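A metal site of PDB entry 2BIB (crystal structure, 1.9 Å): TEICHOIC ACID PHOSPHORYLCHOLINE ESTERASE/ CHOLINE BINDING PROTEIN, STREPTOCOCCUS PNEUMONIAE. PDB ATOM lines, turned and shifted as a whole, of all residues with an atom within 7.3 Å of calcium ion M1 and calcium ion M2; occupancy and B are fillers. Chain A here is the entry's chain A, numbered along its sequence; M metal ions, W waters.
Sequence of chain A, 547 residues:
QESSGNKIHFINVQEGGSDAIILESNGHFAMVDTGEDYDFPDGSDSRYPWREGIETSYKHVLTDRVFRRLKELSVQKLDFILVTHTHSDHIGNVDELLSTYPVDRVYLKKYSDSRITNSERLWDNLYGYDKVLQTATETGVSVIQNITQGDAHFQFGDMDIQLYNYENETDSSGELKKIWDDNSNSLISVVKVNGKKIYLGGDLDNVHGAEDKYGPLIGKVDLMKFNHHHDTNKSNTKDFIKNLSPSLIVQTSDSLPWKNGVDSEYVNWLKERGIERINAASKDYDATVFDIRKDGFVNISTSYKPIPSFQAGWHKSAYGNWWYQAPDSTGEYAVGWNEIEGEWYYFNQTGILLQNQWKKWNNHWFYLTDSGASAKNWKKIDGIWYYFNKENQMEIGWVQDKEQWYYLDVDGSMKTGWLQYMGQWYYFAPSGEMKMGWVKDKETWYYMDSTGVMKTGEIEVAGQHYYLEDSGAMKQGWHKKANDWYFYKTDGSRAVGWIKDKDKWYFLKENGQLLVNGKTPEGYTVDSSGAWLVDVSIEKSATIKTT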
ATOM      1  N   THR A  34       6.862   9.352  17.033  1.00  0.00           N
ATOM      2  CA  THR A  34       5.561   9.665  16.390  1.00  0.00           C
ATOM      3  C   THR A  34       4.866  10.915  16.952  1.00  0.00           C
ATOM      4  O   THR A  34       3.743  11.217  16.544  1.00  0.00           O
ATOM      5  CB  THR A  34       4.620   8.456  16.516  1.00  0.00           C
ATOM      6  OG1 THR A  34       4.216   8.284  17.891  1.00  0.00           O
ATOM      7  CG2 THR A  34       5.314   7.219  16.017  1.00  0.00           C
ATOM      8  N   GLY A  35       5.529  11.618  17.858  1.00  0.00           N
ATOM      9  CA  GLY A  35       4.993  12.831  18.433  1.00  0.00           C
ATOM     10  C   GLY A  35       3.907  12.666  19.473  1.00  0.00           C
ATOM     11  O   GLY A  35       3.379  11.570  19.681  1.00  0.00           O
ATOM     12  N   GLU A  36       3.561  13.762  20.139  1.00  0.00           N
ATOM     13  CA  GLU A  36       2.476  13.791  21.116  1.00  0.00           C
ATOM     14  C   GLU A  36       1.121  13.570  20.464  1.00  0.00           C
ATOM     15  O   GLU A  36       0.854  14.085  19.359  1.00  0.00           O
ATOM     16  CB  GLU A  36       2.468  15.150  21.869  1.00  0.00           C
ATOM     17  CG  GLU A  36       1.483  15.225  23.035  1.00  0.00           C
ATOM     18  CD  GLU A  36       1.830  14.226  24.139  1.00  0.00           C
ATOM     19  OE1 GLU A  36       2.874  14.427  24.794  1.00  0.00           O
ATOM     20  OE2 GLU A  36       1.054  13.239  24.335  1.00  0.00           O
ATOM     21  N   ASP A  37       0.273  12.784  21.133  1.00  0.00           N
ATOM     22  CA  ASP A  37      -1.099  12.512  20.692  1.00  0.00           C
ATOM     23  C   ASP A  37      -2.123  13.183  21.590  1.00  0.00           C
ATOM     24  O   ASP A  37      -1.845  13.433  22.778  1.00  0.00           O
ATOM     25  CB  ASP A  37      -1.410  11.012  20.637  1.00  0.00           C
ATOM     26  CG  ASP A  37      -1.438  10.348  22.025  1.00  0.00           C
ATOM     27  OD1 ASP A  37      -0.774  10.832  22.973  1.00  0.00           O
ATOM     28  OD2 ASP A  37      -2.088   9.305  22.249  1.00  0.00           O
ATOM     29  N   TYR A  38      -3.309  13.434  21.037  1.00  0.00           N
ATOM     30  CA  TYR A  38      -4.451  13.901  21.820  1.00  0.00           C
ATOM     31  C   TYR A  38      -4.732  13.069  23.064  1.00  0.00           C
ATOM     32  O   TYR A  38      -4.915  13.611  24.158  1.00  0.00           O
ATOM     33  CB  TYR A  38      -5.701  13.888  20.940  1.00  0.00           C
ATOM     34  CG  TYR A  38      -5.716  15.004  19.949  1.00  0.00           C
ATOM     35  CD1 TYR A  38      -5.519  14.748  18.596  1.00  0.00           C
ATOM     36  CD2 TYR A  38      -5.937  16.319  20.352  1.00  0.00           C
ATOM     37  CE1 TYR A  38      -5.535  15.784  17.661  1.00  0.00           C
ATOM     38  CE2 TYR A  38      -5.952  17.358  19.431  1.00  0.00           C
ATOM     39  CZ  TYR A  38      -5.759  17.075  18.087  1.00  0.00           C
ATOM     40  OH  TYR A  38      -5.775  18.090  17.167  1.00  0.00           O
ATOM     41  N   ASP A  39      -4.761  11.754  22.886  1.00  0.00           N
ATOM     42  CA  ASP A  39      -5.134  10.822  23.942  1.00  0.00           C
ATOM     43  C   ASP A  39      -4.266  10.944  25.188  1.00  0.00           C
ATOM     44  O   ASP A  39      -3.093  11.323  25.110  1.00  0.00           O
ATOM     45  CB  ASP A  39      -5.116   9.378  23.417  1.00  0.00           C
ATOM     46  CG  ASP A  39      -5.963   8.450  24.252  1.00  0.00           C
ATOM     47  OD1 ASP A  39      -5.765   7.212  24.159  1.00  0.00           O
ATOM     48  OD2 ASP A  39      -6.854   8.856  25.023  1.00  0.00           O
ATOM     49  N   PHE A  40      -4.860  10.595  26.322  1.00  0.00           N
ATOM     50  CA  PHE A  40      -4.156  10.527  27.614  1.00  0.00           C
ATOM     51  C   PHE A  40      -5.035   9.724  28.572  1.00  0.00           C
ATOM     52  O   PHE A  40      -6.244   9.657  28.341  1.00  0.00           O
ATOM     53  CB  PHE A  40      -3.944  11.944  28.169  1.00  0.00           C
ATOM     54  CG  PHE A  40      -5.227  12.731  28.338  1.00  0.00           C
ATOM     55  CD1 PHE A  40      -5.937  12.694  29.546  1.00  0.00           C
ATOM     56  CD2 PHE A  40      -5.708  13.514  27.302  1.00  0.00           C
ATOM     57  CE1 PHE A  40      -7.116  13.416  29.710  1.00  0.00           C
ATOM     58  CE2 PHE A  40      -6.887  14.257  27.453  1.00  0.00           C
ATOM     59  CZ  PHE A  40      -7.591  14.207  28.656  1.00  0.00           C
ATOM     60  N   PRO A  41      -4.482   9.119  29.629  1.00  0.00           N
ATOM     61  CA  PRO A  41      -5.315   8.447  30.625  1.00  0.00           C
ATOM     62  C   PRO A  41      -5.911   9.431  31.627  1.00  0.00           C
ATOM     63  O   PRO A  41      -5.210  10.331  32.073  1.00  0.00           O
ATOM     64  CB  PRO A  41      -4.332   7.482  31.315  1.00  0.00           C
ATOM     65  CG  PRO A  41      -2.966   8.094  31.116  1.00  0.00           C
ATOM     66  CD  PRO A  41      -3.043   9.030  29.925  1.00  0.00           C
ATOM     67  N   ILE A  54       1.059  14.972  33.156  1.00  0.00           N
ATOM     68  CA  ILE A  54       0.592  14.277  31.942  1.00  0.00           C
ATOM     69  C   ILE A  54       0.092  15.332  30.937  1.00  0.00           C
ATOM     70  O   ILE A  54      -0.718  16.200  31.308  1.00  0.00           O
ATOM     71  CB  ILE A  54      -0.535  13.261  32.250  1.00  0.00           C
ATOM     72  CG1 ILE A  54       0.002  12.040  33.025  1.00  0.00           C
ATOM     73  CG2 ILE A  54      -1.259  12.823  30.961  1.00  0.00           C
ATOM     74  CD1 ILE A  54      -1.103  11.123  33.553  1.00  0.00           C
ATOM     75  N   GLU A  55       0.562  15.256  29.694  1.00  0.00           N
ATOM     76  CA  GLU A  55       0.173  16.224  28.631  1.00  0.00           C
ATOM     77  C   GLU A  55      -1.331  16.207  28.268  1.00  0.00           C
ATOM     78  O   GLU A  55      -1.882  15.144  27.959  1.00  0.00           O
ATOM     79  CB  GLU A  55       1.006  15.991  27.359  1.00  0.00           C
ATOM     80  CG  GLU A  55       0.830  17.051  26.280  1.00  0.00           C
ATOM     81  CD  GLU A  55       1.289  18.407  26.764  1.00  0.00           C
ATOM     82  OE1 GLU A  55       2.515  18.644  26.790  1.00  0.00           O
ATOM     83  OE2 GLU A  55       0.440  19.204  27.160  1.00  0.00           O
ATOM     84  N   THR A  56      -1.980  17.373  28.297  1.00  0.00           N
ATOM     85  CA  THR A  56      -3.360  17.528  27.776  1.00  0.00           C
ATOM     86  C   THR A  56      -3.567  18.787  26.909  1.00  0.00           C
ATOM     87  O   THR A  56      -4.710  19.093  26.508  1.00  0.00           O
ATOM     88  CB  THR A  56      -4.414  17.572  28.917  1.00  0.00           C
ATOM     89  OG1 THR A  56      -4.181  18.726  29.729  1.00  0.00           O
ATOM     90  CG2 THR A  56      -4.290  16.375  29.886  1.00  0.00           C
ATOM     91  N   VAL A  61       0.173  18.873  20.927  1.00  0.00           N
ATOM     92  CA  VAL A  61      -0.253  17.676  20.158  1.00  0.00           C
ATOM     93  C   VAL A  61       0.256  17.700  18.709  1.00  0.00           C
ATOM     94  O   VAL A  61       0.021  18.673  17.960  1.00  0.00           O
ATOM     95  CB  VAL A  61      -1.796  17.510  20.173  1.00  0.00           C
ATOM     96  CG1 VAL A  61      -2.258  16.328  19.297  1.00  0.00           C
ATOM     97  CG2 VAL A  61      -2.296  17.334  21.582  1.00  0.00           C
ATOM     98  N   THR A  63      -0.488  15.174  16.490  1.00  0.00           N
ATOM     99  CA  THR A  63      -1.323  14.257  15.697  1.00  0.00           C
ATOM    100  C   THR A  63      -1.729  14.835  14.324  1.00  0.00           C
ATOM    101  O   THR A  63      -1.516  14.187  13.308  1.00  0.00           O
ATOM    102  CB  THR A  63      -2.579  13.861  16.492  1.00  0.00           C
ATOM    103  OG1 THR A  63      -2.208  13.170  17.702  1.00  0.00           O
ATOM    104  CG2 THR A  63      -3.417  12.847  15.701  1.00  0.00           C
ATOM    105  N   SER A  88       5.134  10.337  26.238  1.00  0.00           N
ATOM    106  CA  SER A  88       3.995  10.608  25.380  1.00  0.00           C
ATOM    107  C   SER A  88       4.363  11.437  24.141  1.00  0.00           C
ATOM    108  O   SER A  88       3.751  11.293  23.094  1.00  0.00           O
ATOM    109  CB  SER A  88       2.899  11.315  26.179  1.00  0.00           C
ATOM    110  OG  SER A  88       3.313  12.620  26.547  1.00  0.00           O
ATOM    111  N   ASP A  89       5.359  12.312  24.264  1.00  0.00           N
ATOM    112  CA  ASP A  89       5.734  13.215  23.172  1.00  0.00           C
ATOM    113  C   ASP A  89       6.606  12.532  22.105  1.00  0.00           C
ATOM    114  O   ASP A  89       7.031  13.174  21.134  1.00  0.00           O
ATOM    115  CB  ASP A  89       6.402  14.504  23.685  1.00  0.00           C
ATOM    116  CG  ASP A  89       7.678  14.244  24.468  1.00  0.00           C
ATOM    117  OD1 ASP A  89       7.612  13.465  25.440  1.00  0.00           O
ATOM    118  OD2 ASP A  89       8.795  14.759  24.191  1.00  0.00           O
ATOM    119  N   ILE A  91       6.119   8.478  21.859  1.00  0.00           N
ATOM    120  CA  ILE A  91       5.315   7.272  21.600  1.00  0.00           C
ATOM    121  C   ILE A  91       3.842   7.565  21.290  1.00  0.00           C
ATOM    122  O   ILE A  91       3.077   6.670  20.927  1.00  0.00           O
ATOM    123  CB  ILE A  91       5.418   6.336  22.856  1.00  0.00           C
ATOM    124  CG1 ILE A  91       5.248   4.844  22.488  1.00  0.00           C
ATOM    125  CG2 ILE A  91       4.448   6.807  23.981  1.00  0.00           C
ATOM    126  CD1 ILE A  91       5.703   3.847  23.639  1.00  0.00           C
ATOM    127  N   GLY A  92       3.437   8.825  21.428  1.00  0.00           N
ATOM    128  CA  GLY A  92       2.029   9.179  21.461  1.00  0.00           C
ATOM    129  C   GLY A  92       1.154   8.676  20.333  1.00  0.00           C
ATOM    130  O   GLY A  92       0.080   8.107  20.589  1.00  0.00           O
ATOM    131  N   ASN A  93       1.581   8.883  19.095  1.00  0.00           N
ATOM    132  CA  ASN A  93       0.753   8.477  17.956  1.00  0.00           C
ATOM    133  C   ASN A  93       0.976   7.076  17.379  1.00  0.00           C
ATOM    134  O   ASN A  93       0.446   6.773  16.314  1.00  0.00           O
ATOM    135  CB  ASN A  93       0.823   9.510  16.855  1.00  0.00           C
ATOM    136  CG  ASN A  93       0.213  10.807  17.271  1.00  0.00           C
ATOM    137  OD1 ASN A  93      -0.992  10.901  17.463  1.00  0.00           O
ATOM    138  ND2 ASN A  93       1.049  11.827  17.449  1.00  0.00           N
ATOM    139  N   VAL A  94       1.726   6.231  18.068  1.00  0.00           N
ATOM    140  CA  VAL A  94       2.033   4.898  17.526  1.00  0.00           C
ATOM    141  C   VAL A  94       0.773   4.077  17.305  1.00  0.00           C
ATOM    142  O   VAL A  94       0.580   3.520  16.229  1.00  0.00           O
ATOM    143  CB  VAL A  94       2.998   4.081  18.398  1.00  0.00           C
ATOM    144  CG1 VAL A  94       3.268   2.713  17.750  1.00  0.00           C
ATOM    145  CG2 VAL A  94       4.324   4.826  18.596  1.00  0.00           C
ATOM    146  N   ASP A  95      -0.081   3.994  18.332  1.00  0.00           N
ATOM    147  CA  ASP A  95      -1.282   3.177  18.190  1.00  0.00           C
ATOM    148  C   ASP A  95      -2.205   3.723  17.100  1.00  0.00           C
ATOM    149  O   ASP A  95      -2.732   2.957  16.291  1.00  0.00           O
ATOM    150  CB  ASP A  95      -2.007   2.977  19.526  1.00  0.00           C
ATOM    151  CG  ASP A  95      -2.390   4.278  20.201  1.00  0.00           C
ATOM    152  OD1 ASP A  95      -1.478   5.075  20.524  1.00  0.00           O
ATOM    153  OD2 ASP A  95      -3.576   4.550  20.476  1.00  0.00           O
ATOM    154  N   GLU A  96      -2.378   5.050  17.058  1.00  0.00           N
ATOM    155  CA  GLU A  96      -3.190   5.670  15.991  1.00  0.00           C
ATOM    156  C   GLU A  96      -2.607   5.351  14.600  1.00  0.00           C
ATOM    157  O   GLU A  96      -3.347   5.082  13.651  1.00  0.00           O
ATOM    158  CB  GLU A  96      -3.270   7.185  16.197  1.00  0.00           C
ATOM    159  CG  GLU A  96      -4.092   7.633  17.406  1.00  0.00           C
ATOM    160  CD  GLU A  96      -3.295   7.649  18.719  1.00  0.00           C
ATOM    161  OE1 GLU A  96      -2.076   7.305  18.720  1.00  0.00           O
ATOM    162  OE2 GLU A  96      -3.893   7.989  19.762  1.00  0.00           O
ATOM    163  N   LEU A  97      -1.283   5.361  14.481  1.00  0.00           N
ATOM    164  CA  LEU A  97      -0.631   5.006  13.210  1.00  0.00           C
ATOM    165  C   LEU A  97      -0.842   3.544  12.841  1.00  0.00           C
ATOM    166  O   LEU A  97      -1.151   3.233  11.674  1.00  0.00           O
ATOM    167  CB  LEU A  97       0.858   5.351  13.243  1.00  0.00           C
ATOM    168  CG  LEU A  97       1.140   6.859  13.110  1.00  0.00           C
ATOM    169  CD1 LEU A  97       2.500   7.197  13.724  1.00  0.00           C
ATOM    170  CD2 LEU A  97       1.046   7.320  11.652  1.00  0.00           C
ATOM    171  N   ASP A 124       2.212   9.220  32.066  1.00  0.00           N
ATOM    172  CA  ASP A 124       1.469   8.204  31.317  1.00  0.00           C
ATOM    173  C   ASP A 124       2.377   7.356  30.408  1.00  0.00           C
ATOM    174  O   ASP A 124       1.979   6.972  29.305  1.00  0.00           O
ATOM    175  CB  ASP A 124       0.377   8.854  30.467  1.00  0.00           C
ATOM    176  CG  ASP A 124       0.910   9.910  29.505  1.00  0.00           C
ATOM    177  OD1 ASP A 124       2.068  10.381  29.643  1.00  0.00           O
ATOM    178  OD2 ASP A 124       0.218  10.297  28.548  1.00  0.00           O
ATOM    179  N   TYR A 127       0.818   3.793  29.988  1.00  0.00           N
ATOM    180  CA  TYR A 127      -0.338   3.904  29.101  1.00  0.00           C
ATOM    181  C   TYR A 127       0.098   3.909  27.631  1.00  0.00           C
ATOM    182  O   TYR A 127      -0.477   3.177  26.798  1.00  0.00           O
ATOM    183  CB  TYR A 127      -1.172   5.136  29.450  1.00  0.00           C
ATOM    184  CG  TYR A 127      -2.423   5.272  28.611  1.00  0.00           C
ATOM    185  CD1 TYR A 127      -3.573   4.525  28.891  1.00  0.00           C
ATOM    186  CD2 TYR A 127      -2.468   6.166  27.537  1.00  0.00           C
ATOM    187  CE1 TYR A 127      -4.739   4.643  28.106  1.00  0.00           C
ATOM    188  CE2 TYR A 127      -3.623   6.308  26.766  1.00  0.00           C
ATOM    189  CZ  TYR A 127      -4.758   5.549  27.057  1.00  0.00           C
ATOM    190  OH  TYR A 127      -5.890   5.691  26.271  1.00  0.00           O
ATOM    191  N   GLY A 128       1.136   4.670  27.321  1.00  0.00           N
ATOM    192  CA  GLY A 128       1.597   4.800  25.958  1.00  0.00           C
ATOM    193  C   GLY A 128       2.247   3.520  25.460  1.00  0.00           C
ATOM    194  O   GLY A 128       2.041   3.105  24.316  1.00  0.00           O
ATOM    195  N   LYS A 131      -0.372   0.728  24.879  1.00  0.00           N
ATOM    196  CA  LYS A 131      -1.073   1.052  23.652  1.00  0.00           C
ATOM    197  C   LYS A 131      -0.340   0.488  22.455  1.00  0.00           C
ATOM    198  O   LYS A 131      -0.984  -0.016  21.527  1.00  0.00           O
ATOM    199  CB  LYS A 131      -1.207   2.576  23.515  1.00  0.00           C
ATOM    200  CG  LYS A 131      -2.464   3.196  24.110  1.00  0.00           C
ATOM    201  CD  LYS A 131      -3.767   2.673  23.481  1.00  0.00           C
ATOM    202  CE  LYS A 131      -4.977   2.956  24.379  1.00  0.00           C
ATOM    203  NZ  LYS A 131      -6.276   2.875  23.634  1.00  0.00           N
ATOM    204  N   VAL A 335      -8.565  19.240  24.265  1.00  0.00           N
ATOM    205  CA  VAL A 335      -8.835  18.003  25.008  1.00  0.00           C
ATOM    206  C   VAL A 335      -8.506  18.263  26.467  1.00  0.00           C
ATOM    207  O   VAL A 335      -7.718  19.173  26.787  1.00  0.00           O
ATOM    208  CB  VAL A 335      -8.062  16.730  24.451  1.00  0.00           C
ATOM    209  CG1 VAL A 335      -8.547  16.341  23.033  1.00  0.00           C
ATOM    210  CG2 VAL A 335      -6.547  16.899  24.496  1.00  0.00           C
HETATM  211 CA    CA M   1      -1.041  12.368  24.832  1.00  0.00          CA
HETATM  212 CA    CA M   2      -1.961   7.237  21.195  1.00  0.00          CA
HETATM  213  O   HOH W   1      -0.319  10.274  25.872  1.00  0.00           O
HETATM  214  O   HOH W   2      -3.782   6.390  22.486  1.00  0.00           O
HETATM  215  O   HOH W   3      -2.358  14.336  25.353  1.00  0.00           O
HETATM  216  O   HOH W   4      -0.477   6.787  23.112  1.00  0.00           O
HETATM  217  O   HOH W   5      -0.652  12.628  27.175  1.00  0.00           O
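The nearest printed residue that does not touch calcium ion M1 is Tyr 38 (4.1 Å).
Calcium ion M2 is bound by the backbone carbonyl oxygen (O) of Gly 92 (2.3 Å).
Calcium ion M2 is bound by OD1 of Asp 95.
OD2 of Asp 37 binds calcium ion M2, 2.3 Å away.
Water W2 binds calcium ion M2 (2.4 Å).
Water W4 binds calcium ion M2, 2.5 Å away.
The side-chain carboxylate (OE1) of Glu 96 is bound to calcium ion M2, 2.5 Å away.
OE2 of Glu 96 binds calcium ion M2 (2.5 Å).
Calcium ion M1 is bound by the backbone carbonyl oxygen of Asp 39 (2.3 Å), the side-chain carboxylate of Glu 36 (2.3 Å), water W5 (2.4 Å), water W3 (2.4 Å), the side-chain carboxylate of Asp 37 (2.4 Å), water W1 (2.4 Å) and the backbone carbonyl oxygen of Asp 37 (2.4 Å).
Calcium ion M1 has seven donor atoms within binding distance.
Water W3 lies within hydrogen-bond range of the backbone carbonyl oxygen (O) of Glu 55 (2.8 Å) and the backbone carbonyl oxygen (O) of Tyr 38 (2.9 Å).
Water W5 lies within hydrogen-bond range of the side-chain carboxylate (OD2) of Asp 124 and the backbone carbonyl oxygen (O) of Glu 55.
Water W2 lies within hydrogen-bond range of the side-chain carboxylate (OD1) of Asp 39 (2.7 Å) and the side-chain carboxylate (OD2) of Asp 95 (2.7 Å).
Of the 27 residues printed, 4 come within 4 Å of calcium ion M2.
The nearest printed residue that does not touch calcium ion M2 is Asn 93 (4.4 Å).
O of Glu 36 sits at hydrogen-bond distance from N of Thr 63.
The backbone carbonyl oxygen of Glu 36 lies within hydrogen-bond range of the side-chain amide nitrogen of Asn 93, at 3.0 Å.
The backbone NH (N) of Asp 89 lies within hydrogen-bond range of the side-chain carboxylate (OE1) of Glu 36, at 3.3 Å.
The side-chain hydroxyl of Ser 88 sits at hydrogen-bond distance from the side-chain carboxylate of Glu 36 (2.6 Å).
The side-chain carboxylate (OD1) of Asp 39 is in hydrogen-bond range of the side-chain hydroxyl (OH) of Tyr 127 (2.6 Å).
N of Gly 92 lies within hydrogen-bond range of O of Gly 35, at 3.3 Å.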
